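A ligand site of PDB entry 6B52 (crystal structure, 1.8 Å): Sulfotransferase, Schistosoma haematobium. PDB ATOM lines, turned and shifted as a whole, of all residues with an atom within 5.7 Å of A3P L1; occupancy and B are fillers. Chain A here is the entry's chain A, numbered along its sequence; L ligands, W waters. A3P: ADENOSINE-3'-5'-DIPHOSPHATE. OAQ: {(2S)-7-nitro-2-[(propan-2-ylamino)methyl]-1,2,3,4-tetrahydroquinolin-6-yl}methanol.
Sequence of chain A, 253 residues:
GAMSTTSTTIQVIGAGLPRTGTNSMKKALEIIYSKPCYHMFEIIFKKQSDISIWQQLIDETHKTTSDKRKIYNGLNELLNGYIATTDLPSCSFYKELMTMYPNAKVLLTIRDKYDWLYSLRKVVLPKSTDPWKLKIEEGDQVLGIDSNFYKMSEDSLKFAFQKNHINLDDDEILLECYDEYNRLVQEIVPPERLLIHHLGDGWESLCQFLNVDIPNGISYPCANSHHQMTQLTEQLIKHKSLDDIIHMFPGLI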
ATOM      1  N   LEU A  17      14.754  25.640  -5.087  1.00  0.00           N
ATOM      2  CA  LEU A  17      16.053  26.009  -4.536  1.00  0.00           C
ATOM      3  C   LEU A  17      16.841  24.769  -4.084  1.00  0.00           C
ATOM      4  O   LEU A  17      16.259  23.713  -3.863  1.00  0.00           O
ATOM      5  CB  LEU A  17      15.849  26.991  -3.361  1.00  0.00           C
ATOM      6  CG  LEU A  17      15.341  28.387  -3.759  1.00  0.00           C
ATOM      7  CD1 LEU A  17      14.894  29.189  -2.530  1.00  0.00           C
ATOM      8  CD2 LEU A  17      16.416  29.151  -4.526  1.00  0.00           C
ATOM      9  N   PRO A  18      18.165  24.901  -3.946  1.00  0.00           N
ATOM     10  CA  PRO A  18      18.933  23.772  -3.403  1.00  0.00           C
ATOM     11  C   PRO A  18      18.390  23.310  -2.038  1.00  0.00           C
ATOM     12  O   PRO A  18      17.845  24.108  -1.258  1.00  0.00           O
ATOM     13  CB  PRO A  18      20.356  24.333  -3.278  1.00  0.00           C
ATOM     14  CG  PRO A  18      20.227  25.810  -3.409  1.00  0.00           C
ATOM     15  CD  PRO A  18      19.030  26.039  -4.287  1.00  0.00           C
ATOM     16  N   ARG A  19      18.525  22.011  -1.811  1.00  0.00           N
ATOM     17  CA  ARG A  19      18.058  21.276  -0.625  1.00  0.00           C
ATOM     18  C   ARG A  19      16.535  21.183  -0.567  1.00  0.00           C
ATOM     19  O   ARG A  19      15.977  21.027   0.517  1.00  0.00           O
ATOM     20  CB  ARG A  19      18.612  21.868   0.671  1.00  0.00           C
ATOM     21  CG  ARG A  19      20.136  22.066   0.675  1.00  0.00           C
ATOM     22  CD  ARG A  19      20.886  20.809   0.220  1.00  0.00           C
ATOM     23  NE  ARG A  19      20.761  19.666   1.115  1.00  0.00           N
ATOM     24  CZ  ARG A  19      21.232  18.461   0.831  1.00  0.00           C
ATOM     25  NH1 ARG A  19      21.828  18.255  -0.326  1.00  0.00           N
ATOM     26  NH2 ARG A  19      21.086  17.451   1.694  1.00  0.00           N
ATOM     27  N   THR A  20      15.872  21.210  -1.720  1.00  0.00           N
ATOM     28  CA  THR A  20      14.424  21.020  -1.768  1.00  0.00           C
ATOM     29  C   THR A  20      14.051  19.765  -2.541  1.00  0.00           C
ATOM     30  O   THR A  20      12.914  19.632  -2.980  1.00  0.00           O
ATOM     31  CB  THR A  20      13.684  22.230  -2.403  1.00  0.00           C
ATOM     32  OG1 THR A  20      14.141  22.459  -3.746  1.00  0.00           O
ATOM     33  CG2 THR A  20      13.909  23.527  -1.594  1.00  0.00           C
ATOM     34  N   GLY A  21      15.006  18.854  -2.676  1.00  0.00           N
ATOM     35  CA  GLY A  21      14.796  17.617  -3.420  1.00  0.00           C
ATOM     36  C   GLY A  21      15.128  17.692  -4.897  1.00  0.00           C
ATOM     37  O   GLY A  21      14.604  16.899  -5.702  1.00  0.00           O
ATOM     38  N   THR A  22      16.016  18.623  -5.263  1.00  0.00           N
ATOM     39  CA  THR A  22      16.293  18.895  -6.676  1.00  0.00           C
ATOM     40  C   THR A  22      17.010  17.705  -7.331  1.00  0.00           C
ATOM     41  O   THR A  22      16.745  17.412  -8.494  1.00  0.00           O
ATOM     42  CB  THR A  22      17.146  20.148  -6.885  1.00  0.00           C
ATOM     43  OG1 THR A  22      18.393  19.998  -6.212  1.00  0.00           O
ATOM     44  CG2 THR A  22      16.399  21.402  -6.354  1.00  0.00           C
ATOM     45  N   ASN A  23      17.906  17.057  -6.593  1.00  0.00           N
ATOM     46  CA  ASN A  23      18.641  15.920  -7.141  1.00  0.00           C
ATOM     47  C   ASN A  23      17.733  14.713  -7.357  1.00  0.00           C
ATOM     48  O   ASN A  23      17.863  13.996  -8.357  1.00  0.00           O
ATOM     49  CB  ASN A  23      19.821  15.524  -6.243  1.00  0.00           C
ATOM     50  CG  ASN A  23      20.715  14.490  -6.895  1.00  0.00           C
ATOM     51  OD1 ASN A  23      20.579  13.288  -6.642  1.00  0.00           O
ATOM     52  ND2 ASN A  23      21.620  14.931  -7.756  1.00  0.00           N
ATOM     53  N   SER A  24      16.808  14.480  -6.423  1.00  0.00           N
ATOM     54  CA  SER A  24      15.789  13.442  -6.628  1.00  0.00           C
ATOM     55  C   SER A  24      14.910  13.790  -7.839  1.00  0.00           C
ATOM     56  O   SER A  24      14.565  12.917  -8.614  1.00  0.00           O
ATOM     57  CB  SER A  24      14.919  13.265  -5.371  1.00  0.00           C
ATOM     58  OG  SER A  24      15.676  12.727  -4.311  1.00  0.00           O
ATOM     59  N   HIS A  39      21.813  19.858 -13.136  1.00  0.00           N
ATOM     60  CA  HIS A  39      21.806  19.945 -11.677  1.00  0.00           C
ATOM     61  C   HIS A  39      23.184  20.416 -11.276  1.00  0.00           C
ATOM     62  O   HIS A  39      24.113  20.289 -12.077  1.00  0.00           O
ATOM     63  CB  HIS A  39      21.465  18.596 -11.046  1.00  0.00           C
ATOM     64  CG  HIS A  39      21.251  18.645  -9.566  1.00  0.00           C
ATOM     65  ND1 HIS A  39      22.268  18.432  -8.653  1.00  0.00           N
ATOM     66  CD2 HIS A  39      20.121  18.846  -8.834  1.00  0.00           C
ATOM     67  CE1 HIS A  39      21.785  18.521  -7.428  1.00  0.00           C
ATOM     68  NE2 HIS A  39      20.486  18.762  -7.502  1.00  0.00           N
ATOM     69  N   ASP A  87      17.953  22.853  -9.679  1.00  0.00           N
ATOM     70  CA  ASP A  87      18.982  23.315  -8.759  1.00  0.00           C
ATOM     71  C   ASP A  87      19.639  24.610  -9.232  1.00  0.00           C
ATOM     72  O   ASP A  87      19.468  25.032 -10.379  1.00  0.00           O
ATOM     73  CB  ASP A  87      20.063  22.227  -8.599  1.00  0.00           C
ATOM     74  CG  ASP A  87      20.842  22.328  -7.307  1.00  0.00           C
ATOM     75  OD1 ASP A  87      20.600  23.262  -6.493  1.00  0.00           O
ATOM     76  OD2 ASP A  87      21.699  21.450  -7.113  1.00  0.00           O
ATOM     77  N   ARG A 111       9.780  22.801   0.498  1.00  0.00           N
ATOM     78  CA  ARG A 111       9.701  22.085   1.775  1.00  0.00           C
ATOM     79  C   ARG A 111       9.576  23.097   2.907  1.00  0.00           C
ATOM     80  O   ARG A 111       9.698  24.300   2.671  1.00  0.00           O
ATOM     81  CB  ARG A 111      10.931  21.213   1.992  1.00  0.00           C
ATOM     82  CG  ARG A 111      12.175  22.020   2.302  1.00  0.00           C
ATOM     83  CD  ARG A 111      13.423  21.173   2.374  1.00  0.00           C
ATOM     84  NE  ARG A 111      13.422  20.160   3.430  1.00  0.00           N
ATOM     85  CZ  ARG A 111      14.462  19.371   3.699  1.00  0.00           C
ATOM     86  NH1 ARG A 111      15.580  19.490   2.995  1.00  0.00           N
ATOM     87  NH2 ARG A 111      14.383  18.470   4.658  1.00  0.00           N
ATOM     88  N   ASP A 115      13.429  23.248   8.063  1.00  0.00           N
ATOM     89  CA  ASP A 115      14.113  22.046   7.593  1.00  0.00           C
ATOM     90  C   ASP A 115      15.099  22.400   6.488  1.00  0.00           C
ATOM     91  O   ASP A 115      16.254  21.965   6.506  1.00  0.00           O
ATOM     92  CB  ASP A 115      13.102  21.016   7.086  1.00  0.00           C
ATOM     93  CG  ASP A 115      12.364  20.306   8.213  1.00  0.00           C
ATOM     94  OD1 ASP A 115      12.747  20.477   9.386  1.00  0.00           O
ATOM     95  OD2 ASP A 115      11.388  19.573   7.915  1.00  0.00           O
ATOM     96  N   SER A 119      19.283  22.093   6.489  1.00  0.00           N
ATOM     97  CA  SER A 119      19.889  21.325   5.398  1.00  0.00           C
ATOM     98  C   SER A 119      20.884  22.186   4.614  1.00  0.00           C
ATOM     99  O   SER A 119      22.002  21.762   4.337  1.00  0.00           O
ATOM    100  CB  SER A 119      18.799  20.783   4.465  1.00  0.00           C
ATOM    101  OG  SER A 119      19.376  19.872   3.530  1.00  0.00           O
ATOM    102  N   VAL A 123      25.141  21.589   4.305  1.00  0.00           N
ATOM    103  CA  VAL A 123      25.656  21.083   3.029  1.00  0.00           C
ATOM    104  C   VAL A 123      26.159  22.168   2.082  1.00  0.00           C
ATOM    105  O   VAL A 123      27.244  22.023   1.505  1.00  0.00           O
ATOM    106  CB  VAL A 123      24.564  20.277   2.282  1.00  0.00           C
ATOM    107  CG1 VAL A 123      25.089  19.779   0.946  1.00  0.00           C
ATOM    108  CG2 VAL A 123      24.090  19.117   3.138  1.00  0.00           C
ATOM    109  N   LEU A 199       8.246  17.758  -0.651  1.00  0.00           N
ATOM    110  CA  LEU A 199       9.020  16.570  -0.314  1.00  0.00           C
ATOM    111  C   LEU A 199       8.085  15.440   0.085  1.00  0.00           C
ATOM    112  O   LEU A 199       7.261  15.606   0.977  1.00  0.00           O
ATOM    113  CB  LEU A 199      10.017  16.841   0.819  1.00  0.00           C
ATOM    114  CG  LEU A 199      11.392  17.452   0.512  1.00  0.00           C
ATOM    115  CD1 LEU A 199      12.264  17.494   1.766  1.00  0.00           C
ATOM    116  CD2 LEU A 199      12.113  16.717  -0.617  1.00  0.00           C
ATOM    117  N   GLY A 200       8.220  14.306  -0.589  1.00  0.00           N
ATOM    118  CA  GLY A 200       7.359  13.165  -0.337  1.00  0.00           C
ATOM    119  C   GLY A 200       6.189  13.007  -1.282  1.00  0.00           C
ATOM    120  O   GLY A 200       5.500  11.991  -1.226  1.00  0.00           O
ATOM    121  N   TYR A 220      10.029   6.438  -6.589  1.00  0.00           N
ATOM    122  CA  TYR A 220      10.465   7.821  -6.740  1.00  0.00           C
ATOM    123  C   TYR A 220      11.788   7.994  -5.999  1.00  0.00           C
ATOM    124  O   TYR A 220      11.935   7.491  -4.878  1.00  0.00           O
ATOM    125  CB  TYR A 220       9.417   8.803  -6.188  1.00  0.00           C
ATOM    126  CG  TYR A 220       9.802  10.241  -6.472  1.00  0.00           C
ATOM    127  CD1 TYR A 220      10.601  10.943  -5.583  1.00  0.00           C
ATOM    128  CD2 TYR A 220       9.390  10.880  -7.627  1.00  0.00           C
ATOM    129  CE1 TYR A 220      10.980  12.243  -5.835  1.00  0.00           C
ATOM    130  CE2 TYR A 220       9.753  12.192  -7.887  1.00  0.00           C
ATOM    131  CZ  TYR A 220      10.543  12.863  -6.980  1.00  0.00           C
ATOM    132  OH  TYR A 220      10.931  14.155  -7.213  1.00  0.00           O
ATOM    133  N   PRO A 221      12.767   8.677  -6.620  1.00  0.00           N
ATOM    134  CA  PRO A 221      14.098   8.805  -6.018  1.00  0.00           C
ATOM    135  C   PRO A 221      14.116   9.502  -4.669  1.00  0.00           C
ATOM    136  O   PRO A 221      13.361  10.447  -4.431  1.00  0.00           O
ATOM    137  CB  PRO A 221      14.868   9.612  -7.058  1.00  0.00           C
ATOM    138  CG  PRO A 221      14.194   9.240  -8.382  1.00  0.00           C
ATOM    139  CD  PRO A 221      12.727   9.154  -8.014  1.00  0.00           C
ATOM    140  N   CYS A 222      14.999   9.033  -3.794  1.00  0.00           N
ATOM    141  CA  CYS A 222      15.198   9.647  -2.503  1.00  0.00           C
ATOM    142  C   CYS A 222      16.687   9.853  -2.288  1.00  0.00           C
ATOM    143  O   CYS A 222      17.353   9.047  -1.634  1.00  0.00           O
ATOM    144  CB  CYS A 222      14.598   8.778  -1.401  1.00  0.00           C
ATOM    145  SG  CYS A 222      14.554   9.580   0.205  1.00  0.00           S
ATOM    146  N   ALA A 223      17.222  10.927  -2.870  1.00  0.00           N
ATOM    147  CA  ALA A 223      18.663  11.123  -2.958  1.00  0.00           C
ATOM    148  C   ALA A 223      19.153  12.360  -2.207  1.00  0.00           C
ATOM    149  O   ALA A 223      18.373  13.253  -1.889  1.00  0.00           O
ATOM    150  CB  ALA A 223      19.084  11.227  -4.424  1.00  0.00           C
ATOM    151  N   ASN A 224      20.453  12.370  -1.911  1.00  0.00           N
ATOM    152  CA  ASN A 224      21.164  13.591  -1.542  1.00  0.00           C
ATOM    153  C   ASN A 224      20.833  14.104  -0.136  1.00  0.00           C
ATOM    154  O   ASN A 224      20.703  15.309   0.079  1.00  0.00           O
ATOM    155  CB  ASN A 224      20.883  14.669  -2.600  1.00  0.00           C
ATOM    156  CG  ASN A 224      21.932  15.770  -2.642  1.00  0.00           C
ATOM    157  OD1 ASN A 224      22.952  15.705  -1.952  1.00  0.00           O
ATOM    158  ND2 ASN A 224      21.685  16.790  -3.449  1.00  0.00           N
ATOM    159  N   SER A 225      20.689  13.209   0.841  1.00  0.00           N
ATOM    160  CA  SER A 225      20.426  13.644   2.220  1.00  0.00           C
ATOM    161  C   SER A 225      21.644  14.337   2.840  1.00  0.00           C
ATOM    162  O   SER A 225      22.758  14.170   2.368  1.00  0.00           O
ATOM    163  CB  SER A 225      20.012  12.475   3.112  1.00  0.00           C
ATOM    164  OG  SER A 225      21.130  11.671   3.459  1.00  0.00           O
ATOM    165  N   HIS A 226      21.438  15.147   3.883  1.00  0.00           N
ATOM    166  CA  HIS A 226      22.580  15.822   4.496  1.00  0.00           C
ATOM    167  C   HIS A 226      23.487  14.806   5.192  1.00  0.00           C
ATOM    168  O   HIS A 226      24.699  14.997   5.244  1.00  0.00           O
ATOM    169  CB  HIS A 226      22.125  16.932   5.468  1.00  0.00           C
ATOM    170  CG  HIS A 226      21.401  16.432   6.672  1.00  0.00           C
ATOM    171  ND1 HIS A 226      22.005  15.711   7.676  1.00  0.00           N
ATOM    172  CD2 HIS A 226      20.106  16.592   7.061  1.00  0.00           C
ATOM    173  CE1 HIS A 226      21.116  15.425   8.613  1.00  0.00           C
ATOM    174  NE2 HIS A 226      19.962  15.949   8.261  1.00  0.00           N
ATOM    175  N   HIS A 227      22.883  13.749   5.719  1.00  0.00           N
ATOM    176  CA  HIS A 227      23.671  12.703   6.376  1.00  0.00           C
ATOM    177  C   HIS A 227      24.670  12.112   5.397  1.00  0.00           C
ATOM    178  O   HIS A 227      25.851  11.964   5.713  1.00  0.00           O
ATOM    179  CB  HIS A 227      22.751  11.616   6.948  1.00  0.00           C
ATOM    180  CG  HIS A 227      23.491  10.440   7.512  1.00  0.00           C
ATOM    181  ND1 HIS A 227      24.027  10.431   8.781  1.00  0.00           N
ATOM    182  CD2 HIS A 227      23.787   9.230   6.973  1.00  0.00           C
ATOM    183  CE1 HIS A 227      24.620   9.275   8.997  1.00  0.00           C
ATOM    184  NE2 HIS A 227      24.479   8.525   7.919  1.00  0.00           N
HETATM  185  P1  A3P L   1      17.894  16.666   4.060  1.00  0.00           P
HETATM  186  O1P A3P L   1      18.067  15.197   4.400  1.00  0.00           O
HETATM  187  O2P A3P L   1      17.101  17.353   5.152  1.00  0.00           O
HETATM  188  O3P A3P L   1      19.239  17.332   3.890  1.00  0.00           O
HETATM  189  P2  A3P L   1      18.606  18.657  -2.887  1.00  0.00           P
HETATM  190  O4P A3P L   1      18.792  17.446  -3.812  1.00  0.00           O
HETATM  191  O5P A3P L   1      17.991  19.818  -3.597  1.00  0.00           O
HETATM  192  O6P A3P L   1      19.965  19.011  -2.334  1.00  0.00           O
HETATM  193  O5' A3P L   1      17.628  18.171  -1.734  1.00  0.00           O
HETATM  194  C5' A3P L   1      18.181  17.369  -0.691  1.00  0.00           C
HETATM  195  C4' A3P L   1      17.143  17.208   0.389  1.00  0.00           C
HETATM  196  O4' A3P L   1      15.925  16.598  -0.123  1.00  0.00           O
HETATM  197  C3' A3P L   1      17.621  16.304   1.464  1.00  0.00           C
HETATM  198  O3' A3P L   1      17.061  16.766   2.702  1.00  0.00           O
HETATM  199  C2' A3P L   1      16.998  15.017   1.095  1.00  0.00           C
HETATM  200  O2' A3P L   1      16.977  14.093   2.169  1.00  0.00           O
HETATM  201  C1' A3P L   1      15.640  15.445   0.676  1.00  0.00           C
HETATM  202  N9  A3P L   1      14.965  14.513  -0.160  1.00  0.00           N
HETATM  203  C8  A3P L   1      15.321  14.169  -1.399  1.00  0.00           C
HETATM  204  N7  A3P L   1      14.444  13.288  -1.901  1.00  0.00           N
HETATM  205  C5  A3P L   1      13.485  13.037  -0.963  1.00  0.00           C
HETATM  206  C6  A3P L   1      12.316  12.217  -0.913  1.00  0.00           C
HETATM  207  N6  A3P L   1      11.942  11.395  -1.998  1.00  0.00           N
HETATM  208  N1  A3P L   1      11.575  12.235   0.223  1.00  0.00           N
HETATM  209  C2  A3P L   1      11.930  12.987   1.262  1.00  0.00           C
HETATM  210  N3  A3P L   1      13.005  13.772   1.238  1.00  0.00           N
HETATM  211  C4  A3P L   1      13.814  13.837   0.156  1.00  0.00           C
HETATM  212  C1  OAQ L   2      25.354  21.585  -3.937  1.00  0.00           C
HETATM  213  C2  OAQ L   2      24.861  22.847  -4.281  1.00  0.00           C
HETATM  214  C3  OAQ L   2      25.657  23.970  -3.965  1.00  0.00           C
HETATM  215  C4  OAQ L   2      26.876  23.807  -3.341  1.00  0.00           C
HETATM  216  C5  OAQ L   2      27.358  22.562  -3.013  1.00  0.00           C
HETATM  217  C6  OAQ L   2      26.592  21.437  -3.317  1.00  0.00           C
HETATM  218  C7  OAQ L   2      28.944  21.169  -1.697  1.00  0.00           C
HETATM  219  C8  OAQ L   2      27.700  20.286  -1.605  1.00  0.00           C
HETATM  220  C9  OAQ L   2      27.047  20.182  -2.974  1.00  0.00           C
HETATM  221  C10 OAQ L   2      23.617  22.897  -4.906  1.00  0.00           C
HETATM  222  C11 OAQ L   2      30.079  20.415  -2.406  1.00  0.00           C
HETATM  223  C12 OAQ L   2      30.899  17.140  -0.722  1.00  0.00           C
HETATM  224  C13 OAQ L   2      30.720  17.765  -3.141  1.00  0.00           C
HETATM  225  C14 OAQ L   2      30.316  18.145  -1.732  1.00  0.00           C
HETATM  226  N1  OAQ L   2      28.592  22.452  -2.358  1.00  0.00           N
HETATM  227  N2  OAQ L   2      25.296  25.243  -4.224  1.00  0.00           N
HETATM  228  N3  OAQ L   2      30.751  19.521  -1.441  1.00  0.00           N
HETATM  229  O1  OAQ L   2      26.109  26.290  -3.595  1.00  0.00           O
HETATM  230  O2  OAQ L   2      24.155  25.640  -5.040  1.00  0.00           O
HETATM  231  O3  OAQ L   2      22.998  21.595  -4.909  1.00  0.00           O
HETATM  232  O   HOH W   1      17.172  13.346   6.481  1.00  0.00           O
HETATM  233  O   HOH W   2      16.073  11.069   3.091  1.00  0.00           O
HETATM  234  O   HOH W   3      17.269  15.164  -3.656  1.00  0.00           O
HETATM  235  O   HOH W   4      13.677  14.677   4.018  1.00  0.00           O
HETATM  236  O   HOH W   5       8.960   9.882  -2.260  1.00  0.00           O
HETATM  237  O   HOH W   6      15.394  15.451   6.014  1.00  0.00           O
HETATM  238  O   HOH W   7      16.785  19.120   7.161  1.00  0.00           O
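N7 of A3P L1 sits at hydrogen-bond distance from OG of Ser 24.
NH2 of Arg 111 is in salt-bridge range of O2P of A3P L1, at 3.0 Å.
O5P of A3P L1 lies within hydrogen-bond range of N of Thr 20 (3.2 Å).
The backbone NH (N) of Thr 22 sits at hydrogen-bond distance from an oxygen (O5P) of A3P L1 (2.8 Å).
O3P of A3P L1 lies within hydrogen-bond range of N of His 226 (3.1 Å).
An oxygen (O3P) of A3P L1 sits at hydrogen-bond distance from the side-chain hydroxyl (OG) of Ser 119, 2.6 Å away.
The backbone NH (N) of Asn 23 sits at hydrogen-bond distance from an oxygen (O4P) of A3P L1 (2.9 Å).
O5' of A3P L1 is in hydrogen-bond range of N of Gly 21, at 2.9 Å.
The backbone carbonyl oxygen (O) of Pro 221 sits at hydrogen-bond distance from a nitrogen (N6) of A3P L1, at 3.0 Å.
The backbone NH of Arg 19 sits at hydrogen-bond distance from an oxygen (O5P) of A3P L1, 2.9 Å away.
NH1 of Arg 19 is in salt-bridge range of O6P of A3P L1 (2.8 Å).
OG1 of Thr 22 is in hydrogen-bond range of O5P of A3P L1.
The side-chain amide nitrogen of Asn 224 sits at hydrogen-bond distance from an oxygen (O4P) of A3P L1 (3.0 Å).
An oxygen (O3) of OAQ L2 sits at hydrogen-bond distance from the side-chain carboxylate of Asp 87, 2.6 Å away.
The side-chain hydroxyl (OG1) of Thr 20 is in hydrogen-bond range of the backbone carbonyl oxygen (O) of Leu 17 (2.5 Å).
The backbone NH (N) of Asn 23 is in hydrogen-bond range of a ring nitrogen (NE2) of His 39, 3.2 Å away.
The guanidinium group (NH2) of Arg 19 is in hydrogen-bond range of the backbone carbonyl oxygen (O) of Asn 224 (2.7 Å).
The backbone carbonyl oxygen of Arg 19 is in hydrogen-bond range of the guanidinium group of Arg 111 (2.9 Å).
OG of Ser 24 is in hydrogen-bond range of O of Pro 221, 3.3 Å away.
The side-chain hydroxyl (OG) of Ser 119 lies within hydrogen-bond range of the guanidinium group (NE) of Arg 19.
OG of Ser 24 lies within hydrogen-bond range of N of Ala 223.
The side-chain hydroxyl (OG1) of Thr 22 sits at hydrogen-bond distance from a ring nitrogen (NE2) of His 39 (2.8 Å).
Pro 18 touches A3P L1 (C to O5P, 3.8 Å).
Leu 199 touches A3P L1.
Tyr 220 touches A3P L1 (CD1 to N6, 3.9 Å).
SG of Cys 222 touches C6 of A3P L1 (3.6 Å).
Ala 223 touches A3P L1 (O to C8, 3.2 Å).
CA of Ser 225 touches O2' of A3P L1, 3.5 Å away.
Within 4 Å of A3P L1: Pro 18, Arg 19, Thr 20, Gly 21, Thr 22, Asn 23, Ser 24, Arg 111, Ser 119, Leu 199, Tyr 220, Pro 221, Cys 222, Ala 223, Asn 224, Ser 225 and His 226.
Water W7 lies within hydrogen-bond range of an oxygen (O2P) of A3P L1 and the backbone carbonyl oxygen (O) of Asp 115.
Water W6 lies within hydrogen-bond range of an oxygen (O2P) of A3P L1 (2.7 Å) and the guanidinium group (NH2) of Arg 111 (3.5 Å).
Water W3 lies within hydrogen-bond range of an oxygen (O4P) of A3P L1 (2.7 Å), the backbone carbonyl oxygen (O) of Ala 223 (2.8 Å) and the backbone NH (N) of Ser 24 (2.9 Å).
Water W2 lies within hydrogen-bond range of an oxygen (O2') of A3P L1 (3.3 Å) and the side-chain sulfur (SG) of Cys 222 (3.6 Å).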
